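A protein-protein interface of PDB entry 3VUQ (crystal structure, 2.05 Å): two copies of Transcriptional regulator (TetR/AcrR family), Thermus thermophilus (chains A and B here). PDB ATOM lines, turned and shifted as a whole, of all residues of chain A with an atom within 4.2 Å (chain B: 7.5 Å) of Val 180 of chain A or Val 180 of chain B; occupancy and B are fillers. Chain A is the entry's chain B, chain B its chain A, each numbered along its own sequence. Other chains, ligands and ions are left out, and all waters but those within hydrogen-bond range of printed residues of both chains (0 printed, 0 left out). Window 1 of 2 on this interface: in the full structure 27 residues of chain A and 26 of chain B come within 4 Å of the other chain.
Met 162 of chain A touches Val 158 of chain B. SD of Met 162 of chain A touches CD1 of Leu 177 of chain B (3.9 Å). Met 162 of chain A touches Leu 181 of chain B (CE to CD2, 3.8 Å). Leu 177 of chain A touches Val 158 of chain B. Leu 150 of chain B touches Glu 179 of chain A. Leu 181 of chain A touches Gly 184 of chain B (O to CA, 3.2 Å). O of Arg 182 of chain A touches CA of Gly 184 of chain B, 3.7 Å away. Lys 183 of chain A touches Arg 182 of chain B. Lys 183 of chain A touches Gly 184 of chain B. Gly 184 of chain A touches Arg 182 of chain B.
NH2 of Arg 147 of chain B is in salt-bridge range of OE2 of Glu 179 of chain A (3.7 Å). NH1 of Arg 147 of chain B is in hydrogen-bond range of O of Lys 183 of chain A (3.2 Å). NH2 of Arg 147 of chain B is in hydrogen-bond range of O of Gly 184 of chain A, 2.9 Å away. The backbone NH of Val 185 of chain B sits at hydrogen-bond distance from the backbone carbonyl oxygen of Leu 181 of chain A. The backbone carbonyl oxygen (O) of Arg 182 of chain A is in hydrogen-bond range of the backbone NH (N) of Val 185 of chain B, 3.3 Å away. The guanidinium group of Arg 182 of chain A is in salt-bridge range of the side-chain carboxylate of Glu 186 of chain B (2.8 Å). N of Gly 184 of chain A lies close to N of Gly 184 of chain B (3.2 Å).
Val 180 of chain A touches its own counterpart, Val 180 of chain B. Leu 181 of chain A touches Gly 184 of chain B, and with the chains exchanged Gly 184 of chain A touches Leu 181 of chain B. Arg 182 of chain A touches Gly 184 of chain B, and with the chains exchanged Gly 184 of chain A touches Arg 182 of chain B. Lys 183 of chain A touches Gly 184 of chain B, and with the chains exchanged Gly 184 of chain A touches Lys 183 of chain B. Positions printed for both chains: 176, 177, 178, 179, 180, 181, 182, 183 and 184.
Printed residues of chain B within 4 Å of Val 180 of chain A: Val 180 and Gly 184. Of the printed residues of chain B, Gly 184 of chain A touches Arg 147, Val 180, Leu 181, Arg 182, Lys 183 and Gly 184. Glu 179 of chain B touches none of the printed residues of chain A. Printed residues of chain A within 4 Å of Gly 184 of chain B: Val 180 (3.6 Å), Leu 181 (3.2 Å), Arg 182 (3.7 Å), Lys 183 (3.6 Å) and Gly 184 (3.2 Å). The nearest printed residue of chain B that does not touch Val 180 of chain A is Leu 181 of chain B (4.01 Å).
Hydrophobic or aromatic side chains of chain B that line the printed part of chain A: Leu 150, Ala 154, Val 158, Leu 177, Leu 181 and Val 185. Hydrophobic or aromatic side chains of chain A that line the printed part of chain B: Met 162, His 176 and Leu 177. Among the printed residues, 26 pairs touch across the chains. Among the printed residues, Asp or Glu carboxylates within 4 Å of a Lys or Arg side-chain nitrogen of the other chain: Glu 179 of chain A with Arg 147 of chain B and Arg 182 of chain A with Glu 186 of chain B.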
ATOM      1  N   MET A 162      -1.264  18.294  -3.248  1.00  0.00           N
ATOM      2  CA  MET A 162      -1.684  16.911  -3.034  1.00  0.00           C
ATOM      3  C   MET A 162      -1.855  16.130  -4.330  1.00  0.00           C
ATOM      4  O   MET A 162      -1.888  14.902  -4.318  1.00  0.00           O
ATOM      5  CB  MET A 162      -2.995  16.860  -2.234  1.00  0.00           C
ATOM      6  CG  MET A 162      -2.836  17.186  -0.747  1.00  0.00           C
ATOM      7  SD  MET A 162      -4.361  16.990   0.222  1.00  0.00           S
ATOM      8  CE  MET A 162      -4.553  15.112   0.182  1.00  0.00           C
ATOM      9  N   HIS A 176      -7.808   6.578  -3.635  1.00  0.00           N
ATOM     10  CA  HIS A 176      -7.466   6.885  -2.251  1.00  0.00           C
ATOM     11  C   HIS A 176      -7.298   8.386  -2.063  1.00  0.00           C
ATOM     12  O   HIS A 176      -7.650   8.920  -1.020  1.00  0.00           O
ATOM     13  CB  HIS A 176      -6.195   6.152  -1.858  1.00  0.00           C
ATOM     14  CG  HIS A 176      -6.383   4.674  -1.724  1.00  0.00           C
ATOM     15  ND1 HIS A 176      -7.078   4.106  -0.679  1.00  0.00           N
ATOM     16  CD2 HIS A 176      -6.004   3.653  -2.526  1.00  0.00           C
ATOM     17  CE1 HIS A 176      -7.121   2.796  -0.843  1.00  0.00           C
ATOM     18  NE2 HIS A 176      -6.477   2.495  -1.957  1.00  0.00           N
ATOM     19  N   LEU A 177      -6.738   9.049  -3.073  1.00  0.00           N
ATOM     20  CA  LEU A 177      -6.572  10.492  -3.033  1.00  0.00           C
ATOM     21  C   LEU A 177      -7.972  11.104  -2.906  1.00  0.00           C
ATOM     22  O   LEU A 177      -8.200  11.977  -2.080  1.00  0.00           O
ATOM     23  CB  LEU A 177      -5.911  10.984  -4.318  1.00  0.00           C
ATOM     24  CG  LEU A 177      -5.859  12.500  -4.570  1.00  0.00           C
ATOM     25  CD1 LEU A 177      -5.153  13.219  -3.407  1.00  0.00           C
ATOM     26  CD2 LEU A 177      -5.130  12.764  -5.875  1.00  0.00           C
ATOM     27  N   MET A 178      -8.913  10.625  -3.719  1.00  0.00           N
ATOM     28  CA  MET A 178     -10.286  11.135  -3.682  1.00  0.00           C
ATOM     29  C   MET A 178     -10.951  10.935  -2.332  1.00  0.00           C
ATOM     30  O   MET A 178     -11.697  11.808  -1.869  1.00  0.00           O
ATOM     31  CB  MET A 178     -11.145  10.468  -4.762  1.00  0.00           C
ATOM     32  CG  MET A 178     -10.724  10.837  -6.177  1.00  0.00           C
ATOM     33  SD  MET A 178     -10.815  12.611  -6.446  1.00  0.00           S
ATOM     34  CE  MET A 178     -12.525  12.869  -6.181  1.00  0.00           C
ATOM     35  N   GLU A 179     -10.726   9.779  -1.710  1.00  0.00           N
ATOM     36  CA  GLU A 179     -11.320   9.528  -0.399  1.00  0.00           C
ATOM     37  C   GLU A 179     -10.761  10.510   0.652  1.00  0.00           C
ATOM     38  O   GLU A 179     -11.502  10.993   1.513  1.00  0.00           O
ATOM     39  CB  GLU A 179     -11.079   8.080   0.041  1.00  0.00           C
ATOM     40  CG  GLU A 179     -11.229   7.880   1.544  1.00  0.00           C
ATOM     41  CD  GLU A 179     -11.381   6.423   1.954  1.00  0.00           C
ATOM     42  OE1 GLU A 179     -10.696   5.549   1.371  1.00  0.00           O
ATOM     43  OE2 GLU A 179     -12.182   6.163   2.881  1.00  0.00           O
ATOM     44  N   VAL A 180      -9.464  10.797   0.588  1.00  0.00           N
ATOM     45  CA  VAL A 180      -8.864  11.751   1.535  1.00  0.00           C
ATOM     46  C   VAL A 180      -9.354  13.175   1.238  1.00  0.00           C
ATOM     47  O   VAL A 180      -9.696  13.929   2.148  1.00  0.00           O
ATOM     48  CB  VAL A 180      -7.313  11.704   1.471  1.00  0.00           C
ATOM     49  CG1 VAL A 180      -6.689  12.847   2.301  1.00  0.00           C
ATOM     50  CG2 VAL A 180      -6.828  10.365   2.016  1.00  0.00           C
ATOM     51  N   LEU A 181      -9.400  13.541  -0.038  1.00  0.00           N
ATOM     52  CA  LEU A 181      -9.861  14.868  -0.426  1.00  0.00           C
ATOM     53  C   LEU A 181     -11.316  15.073  -0.034  1.00  0.00           C
ATOM     54  O   LEU A 181     -11.717  16.167   0.384  1.00  0.00           O
ATOM     55  CB  LEU A 181      -9.708  15.080  -1.939  1.00  0.00           C
ATOM     56  CG  LEU A 181      -8.295  15.273  -2.467  1.00  0.00           C
ATOM     57  CD1 LEU A 181      -8.367  15.497  -3.979  1.00  0.00           C
ATOM     58  CD2 LEU A 181      -7.633  16.453  -1.804  1.00  0.00           C
ATOM     59  N   ARG A 182     -12.116  14.023  -0.158  1.00  0.00           N
ATOM     60  CA  ARG A 182     -13.515  14.164   0.208  1.00  0.00           C
ATOM     61  C   ARG A 182     -13.746  14.186   1.721  1.00  0.00           C
ATOM     62  O   ARG A 182     -14.515  14.998   2.203  1.00  0.00           O
ATOM     63  CB  ARG A 182     -14.359  13.046  -0.419  1.00  0.00           C
ATOM     64  CG  ARG A 182     -15.846  13.176  -0.109  1.00  0.00           C
ATOM     65  CD  ARG A 182     -16.629  11.924  -0.490  1.00  0.00           C
ATOM     66  NE  ARG A 182     -16.679  11.682  -1.931  1.00  0.00           N
ATOM     67  CZ  ARG A 182     -17.772  11.821  -2.678  1.00  0.00           C
ATOM     68  NH1 ARG A 182     -18.916  12.208  -2.127  1.00  0.00           N
ATOM     69  NH2 ARG A 182     -17.728  11.553  -3.974  1.00  0.00           N
ATOM     70  N   LYS A 183     -13.088  13.315   2.485  1.00  0.00           N
ATOM     71  CA  LYS A 183     -13.358  13.310   3.925  1.00  0.00           C
ATOM     72  C   LYS A 183     -12.205  13.258   4.908  1.00  0.00           C
ATOM     73  O   LYS A 183     -12.411  12.995   6.087  1.00  0.00           O
ATOM     74  CB  LYS A 183     -14.355  12.195   4.258  1.00  0.00           C
ATOM     75  CG  LYS A 183     -14.053  10.861   3.625  1.00  0.00           C
ATOM     76  CD  LYS A 183     -15.177   9.880   3.920  1.00  0.00           C
ATOM     77  CE  LYS A 183     -14.913   8.514   3.314  1.00  0.00           C
ATOM     78  NZ  LYS A 183     -16.032   7.567   3.592  1.00  0.00           N
ATOM     79  N   GLY A 184     -10.990  13.519   4.441  1.00  0.00           N
ATOM     80  CA  GLY A 184      -9.850  13.517   5.345  1.00  0.00           C
ATOM     81  C   GLY A 184      -9.611  12.179   6.027  1.00  0.00           C
ATOM     82  O   GLY A 184     -10.068  11.147   5.534  1.00  0.00           O
ATOM     83  N   ARG B 147      -9.329   7.307  11.133  1.00  0.00           N
ATOM     84  CA  ARG B 147     -10.310   6.235  10.976  1.00  0.00           C
ATOM     85  C   ARG B 147      -9.607   4.897  10.801  1.00  0.00           C
ATOM     86  O   ARG B 147      -8.668   4.773  10.010  1.00  0.00           O
ATOM     87  CB  ARG B 147     -11.216   6.478   9.768  1.00  0.00           C
ATOM     88  CG  ARG B 147     -12.080   7.714   9.871  1.00  0.00           C
ATOM     89  CD  ARG B 147     -13.128   7.760   8.750  1.00  0.00           C
ATOM     90  NE  ARG B 147     -12.546   7.755   7.403  1.00  0.00           N
ATOM     91  CZ  ARG B 147     -12.086   8.829   6.767  1.00  0.00           C
ATOM     92  NH1 ARG B 147     -12.123  10.025   7.350  1.00  0.00           N
ATOM     93  NH2 ARG B 147     -11.619   8.712   5.523  1.00  0.00           N
ATOM     94  N   LEU B 150      -9.235   3.280   7.237  1.00  0.00           N
ATOM     95  CA  LEU B 150      -8.202   3.710   6.299  1.00  0.00           C
ATOM     96  C   LEU B 150      -6.991   2.799   6.249  1.00  0.00           C
ATOM     97  O   LEU B 150      -6.485   2.360   7.283  1.00  0.00           O
ATOM     98  CB  LEU B 150      -7.708   5.118   6.656  1.00  0.00           C
ATOM     99  CG  LEU B 150      -8.597   6.304   6.295  1.00  0.00           C
ATOM    100  CD1 LEU B 150      -7.971   7.577   6.847  1.00  0.00           C
ATOM    101  CD2 LEU B 150      -8.741   6.399   4.777  1.00  0.00           C
ATOM    102  N   ALA B 154      -1.973   3.026   1.766  1.00  0.00           N
ATOM    103  CA  ALA B 154      -2.572   3.865   0.733  1.00  0.00           C
ATOM    104  C   ALA B 154      -2.650   5.308   1.186  1.00  0.00           C
ATOM    105  O   ALA B 154      -2.380   6.220   0.411  1.00  0.00           O
ATOM    106  CB  ALA B 154      -3.972   3.363   0.374  1.00  0.00           C
ATOM    107  N   THR B 155      -3.028   5.513   2.442  1.00  0.00           N
ATOM    108  CA  THR B 155      -3.148   6.870   2.956  1.00  0.00           C
ATOM    109  C   THR B 155      -1.784   7.552   3.069  1.00  0.00           C
ATOM    110  O   THR B 155      -1.678   8.747   2.832  1.00  0.00           O
ATOM    111  CB  THR B 155      -3.894   6.879   4.296  1.00  0.00           C
ATOM    112  OG1 THR B 155      -5.128   6.177   4.129  1.00  0.00           O
ATOM    113  CG2 THR B 155      -4.218   8.309   4.731  1.00  0.00           C
ATOM    114  N   ALA B 156      -0.737   6.797   3.408  1.00  0.00           N
ATOM    115  CA  ALA B 156       0.626   7.370   3.478  1.00  0.00           C
ATOM    116  C   ALA B 156       1.049   7.874   2.072  1.00  0.00           C
ATOM    117  O   ALA B 156       1.644   8.940   1.923  1.00  0.00           O
ATOM    118  CB  ALA B 156       1.631   6.286   3.973  1.00  0.00           C
ATOM    119  N   VAL B 158      -0.790   9.003  -0.326  1.00  0.00           N
ATOM    120  CA  VAL B 158      -1.494  10.250  -0.605  1.00  0.00           C
ATOM    121  C   VAL B 158      -0.840  11.417   0.142  1.00  0.00           C
ATOM    122  O   VAL B 158      -0.548  12.463  -0.441  1.00  0.00           O
ATOM    123  CB  VAL B 158      -2.979  10.140  -0.193  1.00  0.00           C
ATOM    124  CG1 VAL B 158      -3.664  11.499  -0.288  1.00  0.00           C
ATOM    125  CG2 VAL B 158      -3.682   9.137  -1.102  1.00  0.00           C
ATOM    126  N   ILE B 159      -0.596  11.243   1.435  1.00  0.00           N
ATOM    127  CA  ILE B 159       0.033  12.304   2.212  1.00  0.00           C
ATOM    128  C   ILE B 159       1.450  12.621   1.713  1.00  0.00           C
ATOM    129  O   ILE B 159       1.873  13.776   1.697  1.00  0.00           O
ATOM    130  CB  ILE B 159       0.047  11.928   3.706  1.00  0.00           C
ATOM    131  CG1 ILE B 159      -1.405  11.871   4.213  1.00  0.00           C
ATOM    132  CG2 ILE B 159       0.881  12.929   4.496  1.00  0.00           C
ATOM    133  CD1 ILE B 159      -1.577  11.339   5.640  1.00  0.00           C
ATOM    134  N   LEU B 174      -0.140  25.795   5.366  1.00  0.00           N
ATOM    135  CA  LEU B 174      -0.141  24.568   6.141  1.00  0.00           C
ATOM    136  C   LEU B 174      -1.434  24.348   6.935  1.00  0.00           C
ATOM    137  O   LEU B 174      -1.903  23.214   7.072  1.00  0.00           O
ATOM    138  CB  LEU B 174       1.067  24.587   7.074  1.00  0.00           C
ATOM    139  CG  LEU B 174       1.572  23.272   7.657  1.00  0.00           C
ATOM    140  CD1 LEU B 174       1.706  22.216   6.562  1.00  0.00           C
ATOM    141  CD2 LEU B 174       2.921  23.538   8.319  1.00  0.00           C
ATOM    142  N   GLU B 175      -2.009  25.428   7.456  1.00  0.00           N
ATOM    143  CA  GLU B 175      -3.238  25.317   8.241  1.00  0.00           C
ATOM    144  C   GLU B 175      -4.391  24.801   7.373  1.00  0.00           C
ATOM    145  O   GLU B 175      -5.223  24.017   7.829  1.00  0.00           O
ATOM    146  CB  GLU B 175      -3.595  26.680   8.856  1.00  0.00           C
ATOM    147  CG  GLU B 175      -2.532  27.268   9.765  1.00  0.00           C
ATOM    148  CD  GLU B 175      -2.750  28.768   9.992  1.00  0.00           C
ATOM    149  OE1 GLU B 175      -2.944  29.493   8.983  1.00  0.00           O
ATOM    150  OE2 GLU B 175      -2.727  29.218  11.164  1.00  0.00           O
ATOM    151  N   HIS B 176      -4.452  25.271   6.130  1.00  0.00           N
ATOM    152  CA  HIS B 176      -5.477  24.827   5.200  1.00  0.00           C
ATOM    153  C   HIS B 176      -5.245  23.360   4.804  1.00  0.00           C
ATOM    154  O   HIS B 176      -6.192  22.577   4.679  1.00  0.00           O
ATOM    155  CB  HIS B 176      -5.469  25.727   3.962  1.00  0.00           C
ATOM    156  CG  HIS B 176      -5.921  27.131   4.239  1.00  0.00           C
ATOM    157  ND1 HIS B 176      -7.253  27.474   4.338  1.00  0.00           N
ATOM    158  CD2 HIS B 176      -5.220  28.281   4.418  1.00  0.00           C
ATOM    159  CE1 HIS B 176      -7.355  28.775   4.560  1.00  0.00           C
ATOM    160  NE2 HIS B 176      -6.137  29.288   4.612  1.00  0.00           N
ATOM    161  N   LEU B 177      -3.989  22.988   4.593  1.00  0.00           N
ATOM    162  CA  LEU B 177      -3.683  21.594   4.244  1.00  0.00           C
ATOM    163  C   LEU B 177      -4.117  20.681   5.408  1.00  0.00           C
ATOM    164  O   LEU B 177      -4.714  19.625   5.192  1.00  0.00           O
ATOM    165  CB  LEU B 177      -2.183  21.414   4.004  1.00  0.00           C
ATOM    166  CG  LEU B 177      -1.653  19.967   3.851  1.00  0.00           C
ATOM    167  CD1 LEU B 177      -2.261  19.282   2.589  1.00  0.00           C
ATOM    168  CD2 LEU B 177      -0.125  20.005   3.718  1.00  0.00           C
ATOM    169  N   MET B 178      -3.801  21.089   6.634  1.00  0.00           N
ATOM    170  CA  MET B 178      -4.163  20.293   7.818  1.00  0.00           C
ATOM    171  C   MET B 178      -5.668  20.156   7.923  1.00  0.00           C
ATOM    172  O   MET B 178      -6.191  19.103   8.310  1.00  0.00           O
ATOM    173  CB  MET B 178      -3.620  20.931   9.088  1.00  0.00           C
ATOM    174  CG  MET B 178      -2.090  20.838   9.226  1.00  0.00           C
ATOM    175  SD  MET B 178      -1.485  19.127   9.149  1.00  0.00           S
ATOM    176  CE  MET B 178      -2.449  18.386  10.483  1.00  0.00           C
ATOM    177  N   GLU B 179      -6.377  21.220   7.569  1.00  0.00           N
ATOM    178  CA  GLU B 179      -7.846  21.192   7.603  1.00  0.00           C
ATOM    179  C   GLU B 179      -8.385  20.160   6.595  1.00  0.00           C
ATOM    180  O   GLU B 179      -9.343  19.441   6.874  1.00  0.00           O
ATOM    181  CB  GLU B 179      -8.384  22.592   7.273  1.00  0.00           C
ATOM    182  CG  GLU B 179      -9.831  22.650   6.848  1.00  0.00           C
ATOM    183  CD  GLU B 179     -10.782  22.713   8.032  1.00  0.00           C
ATOM    184  OE1 GLU B 179     -10.296  22.871   9.179  1.00  0.00           O
ATOM    185  OE2 GLU B 179     -12.011  22.615   7.805  1.00  0.00           O
ATOM    186  N   VAL B 180      -7.787  20.109   5.411  1.00  0.00           N
ATOM    187  CA  VAL B 180      -8.219  19.160   4.387  1.00  0.00           C
ATOM    188  C   VAL B 180      -7.796  17.730   4.784  1.00  0.00           C
ATOM    189  O   VAL B 180      -8.553  16.773   4.640  1.00  0.00           O
ATOM    190  CB  VAL B 180      -7.626  19.543   2.999  1.00  0.00           C
ATOM    191  CG1 VAL B 180      -7.857  18.432   1.999  1.00  0.00           C
ATOM    192  CG2 VAL B 180      -8.290  20.841   2.487  1.00  0.00           C
ATOM    193  N   LEU B 181      -6.593  17.576   5.303  1.00  0.00           N
ATOM    194  CA  LEU B 181      -6.174  16.234   5.695  1.00  0.00           C
ATOM    195  C   LEU B 181      -7.040  15.684   6.818  1.00  0.00           C
ATOM    196  O   LEU B 181      -7.360  14.493   6.866  1.00  0.00           O
ATOM    197  CB  LEU B 181      -4.719  16.241   6.114  1.00  0.00           C
ATOM    198  CG  LEU B 181      -3.773  16.431   4.931  1.00  0.00           C
ATOM    199  CD1 LEU B 181      -2.333  16.496   5.448  1.00  0.00           C
ATOM    200  CD2 LEU B 181      -3.936  15.261   3.948  1.00  0.00           C
ATOM    201  N   ARG B 182      -7.446  16.562   7.717  1.00  0.00           N
ATOM    202  CA  ARG B 182      -8.278  16.139   8.819  1.00  0.00           C
ATOM    203  C   ARG B 182      -9.725  15.842   8.422  1.00  0.00           C
ATOM    204  O   ARG B 182     -10.255  14.782   8.747  1.00  0.00           O
ATOM    205  CB  ARG B 182      -8.269  17.226   9.910  1.00  0.00           C
ATOM    206  CG  ARG B 182      -9.042  16.860  11.177  1.00  0.00           C
ATOM    207  CD  ARG B 182      -9.225  18.075  12.107  1.00  0.00           C
ATOM    208  NE  ARG B 182      -7.991  18.578  12.713  1.00  0.00           N
ATOM    209  CZ  ARG B 182      -7.591  18.278  13.953  1.00  0.00           C
ATOM    210  NH1 ARG B 182      -8.322  17.471  14.703  1.00  0.00           N
ATOM    211  NH2 ARG B 182      -6.484  18.816  14.466  1.00  0.00           N
ATOM    212  N   LYS B 183     -10.348  16.771   7.694  1.00  0.00           N
ATOM    213  CA  LYS B 183     -11.777  16.651   7.361  1.00  0.00           C
ATOM    214  C   LYS B 183     -12.149  16.561   5.882  1.00  0.00           C
ATOM    215  O   LYS B 183     -13.316  16.384   5.567  1.00  0.00           O
ATOM    216  CB  LYS B 183     -12.547  17.863   7.931  1.00  0.00           C
ATOM    217  CG  LYS B 183     -12.134  18.306   9.335  1.00  0.00           C
ATOM    218  CD  LYS B 183     -12.855  17.521  10.412  1.00  0.00           C
ATOM    219  CE  LYS B 183     -14.325  17.931  10.497  1.00  0.00           C
ATOM    220  NZ  LYS B 183     -15.087  17.147  11.518  1.00  0.00           N
ATOM    221  N   GLY B 184     -11.191  16.705   4.976  1.00  0.00           N
ATOM    222  CA  GLY B 184     -11.555  16.660   3.563  1.00  0.00           C
ATOM    223  C   GLY B 184     -12.282  17.950   3.188  1.00  0.00           C
ATOM    224  O   GLY B 184     -12.191  18.956   3.905  1.00  0.00           O
ATOM    225  N   VAL B 185     -13.017  17.938   2.086  1.00  0.00           N
ATOM    226  CA  VAL B 185     -13.725  19.135   1.654  1.00  0.00           C
ATOM    227  C   VAL B 185     -15.258  19.007   1.648  1.00  0.00           C
ATOM    228  O   VAL B 185     -15.954  19.991   1.454  1.00  0.00           O
ATOM    229  CB  VAL B 185     -13.296  19.547   0.245  1.00  0.00           C
ATOM    230  CG1 VAL B 185     -11.773  19.701   0.183  1.00  0.00           C
ATOM    231  CG2 VAL B 185     -13.798  18.512  -0.766  1.00  0.00           C
ATOM    232  N   GLU B 186     -15.773  17.804   1.863  1.00  0.00           N
ATOM    233  CA  GLU B 186     -17.223  17.603   1.842  1.00  0.00           C
ATOM    234  C   GLU B 186     -17.869  18.076   3.136  1.00  0.00           C
ATOM    235  O   GLU B 186     -17.284  17.951   4.204  1.00  0.00           O
ATOM    236  CB  GLU B 186     -17.534  16.122   1.644  1.00  0.00           C
ATOM    237  CG  GLU B 186     -18.794  15.857   0.854  1.00  0.00           C
ATOM    238  CD  GLU B 186     -19.081  14.375   0.708  1.00  0.00           C
ATOM    239  OE1 GLU B 186     -19.892  14.012  -0.169  1.00  0.00           O
ATOM    240  OE2 GLU B 186     -18.500  13.581   1.480  1.00  0.00           O
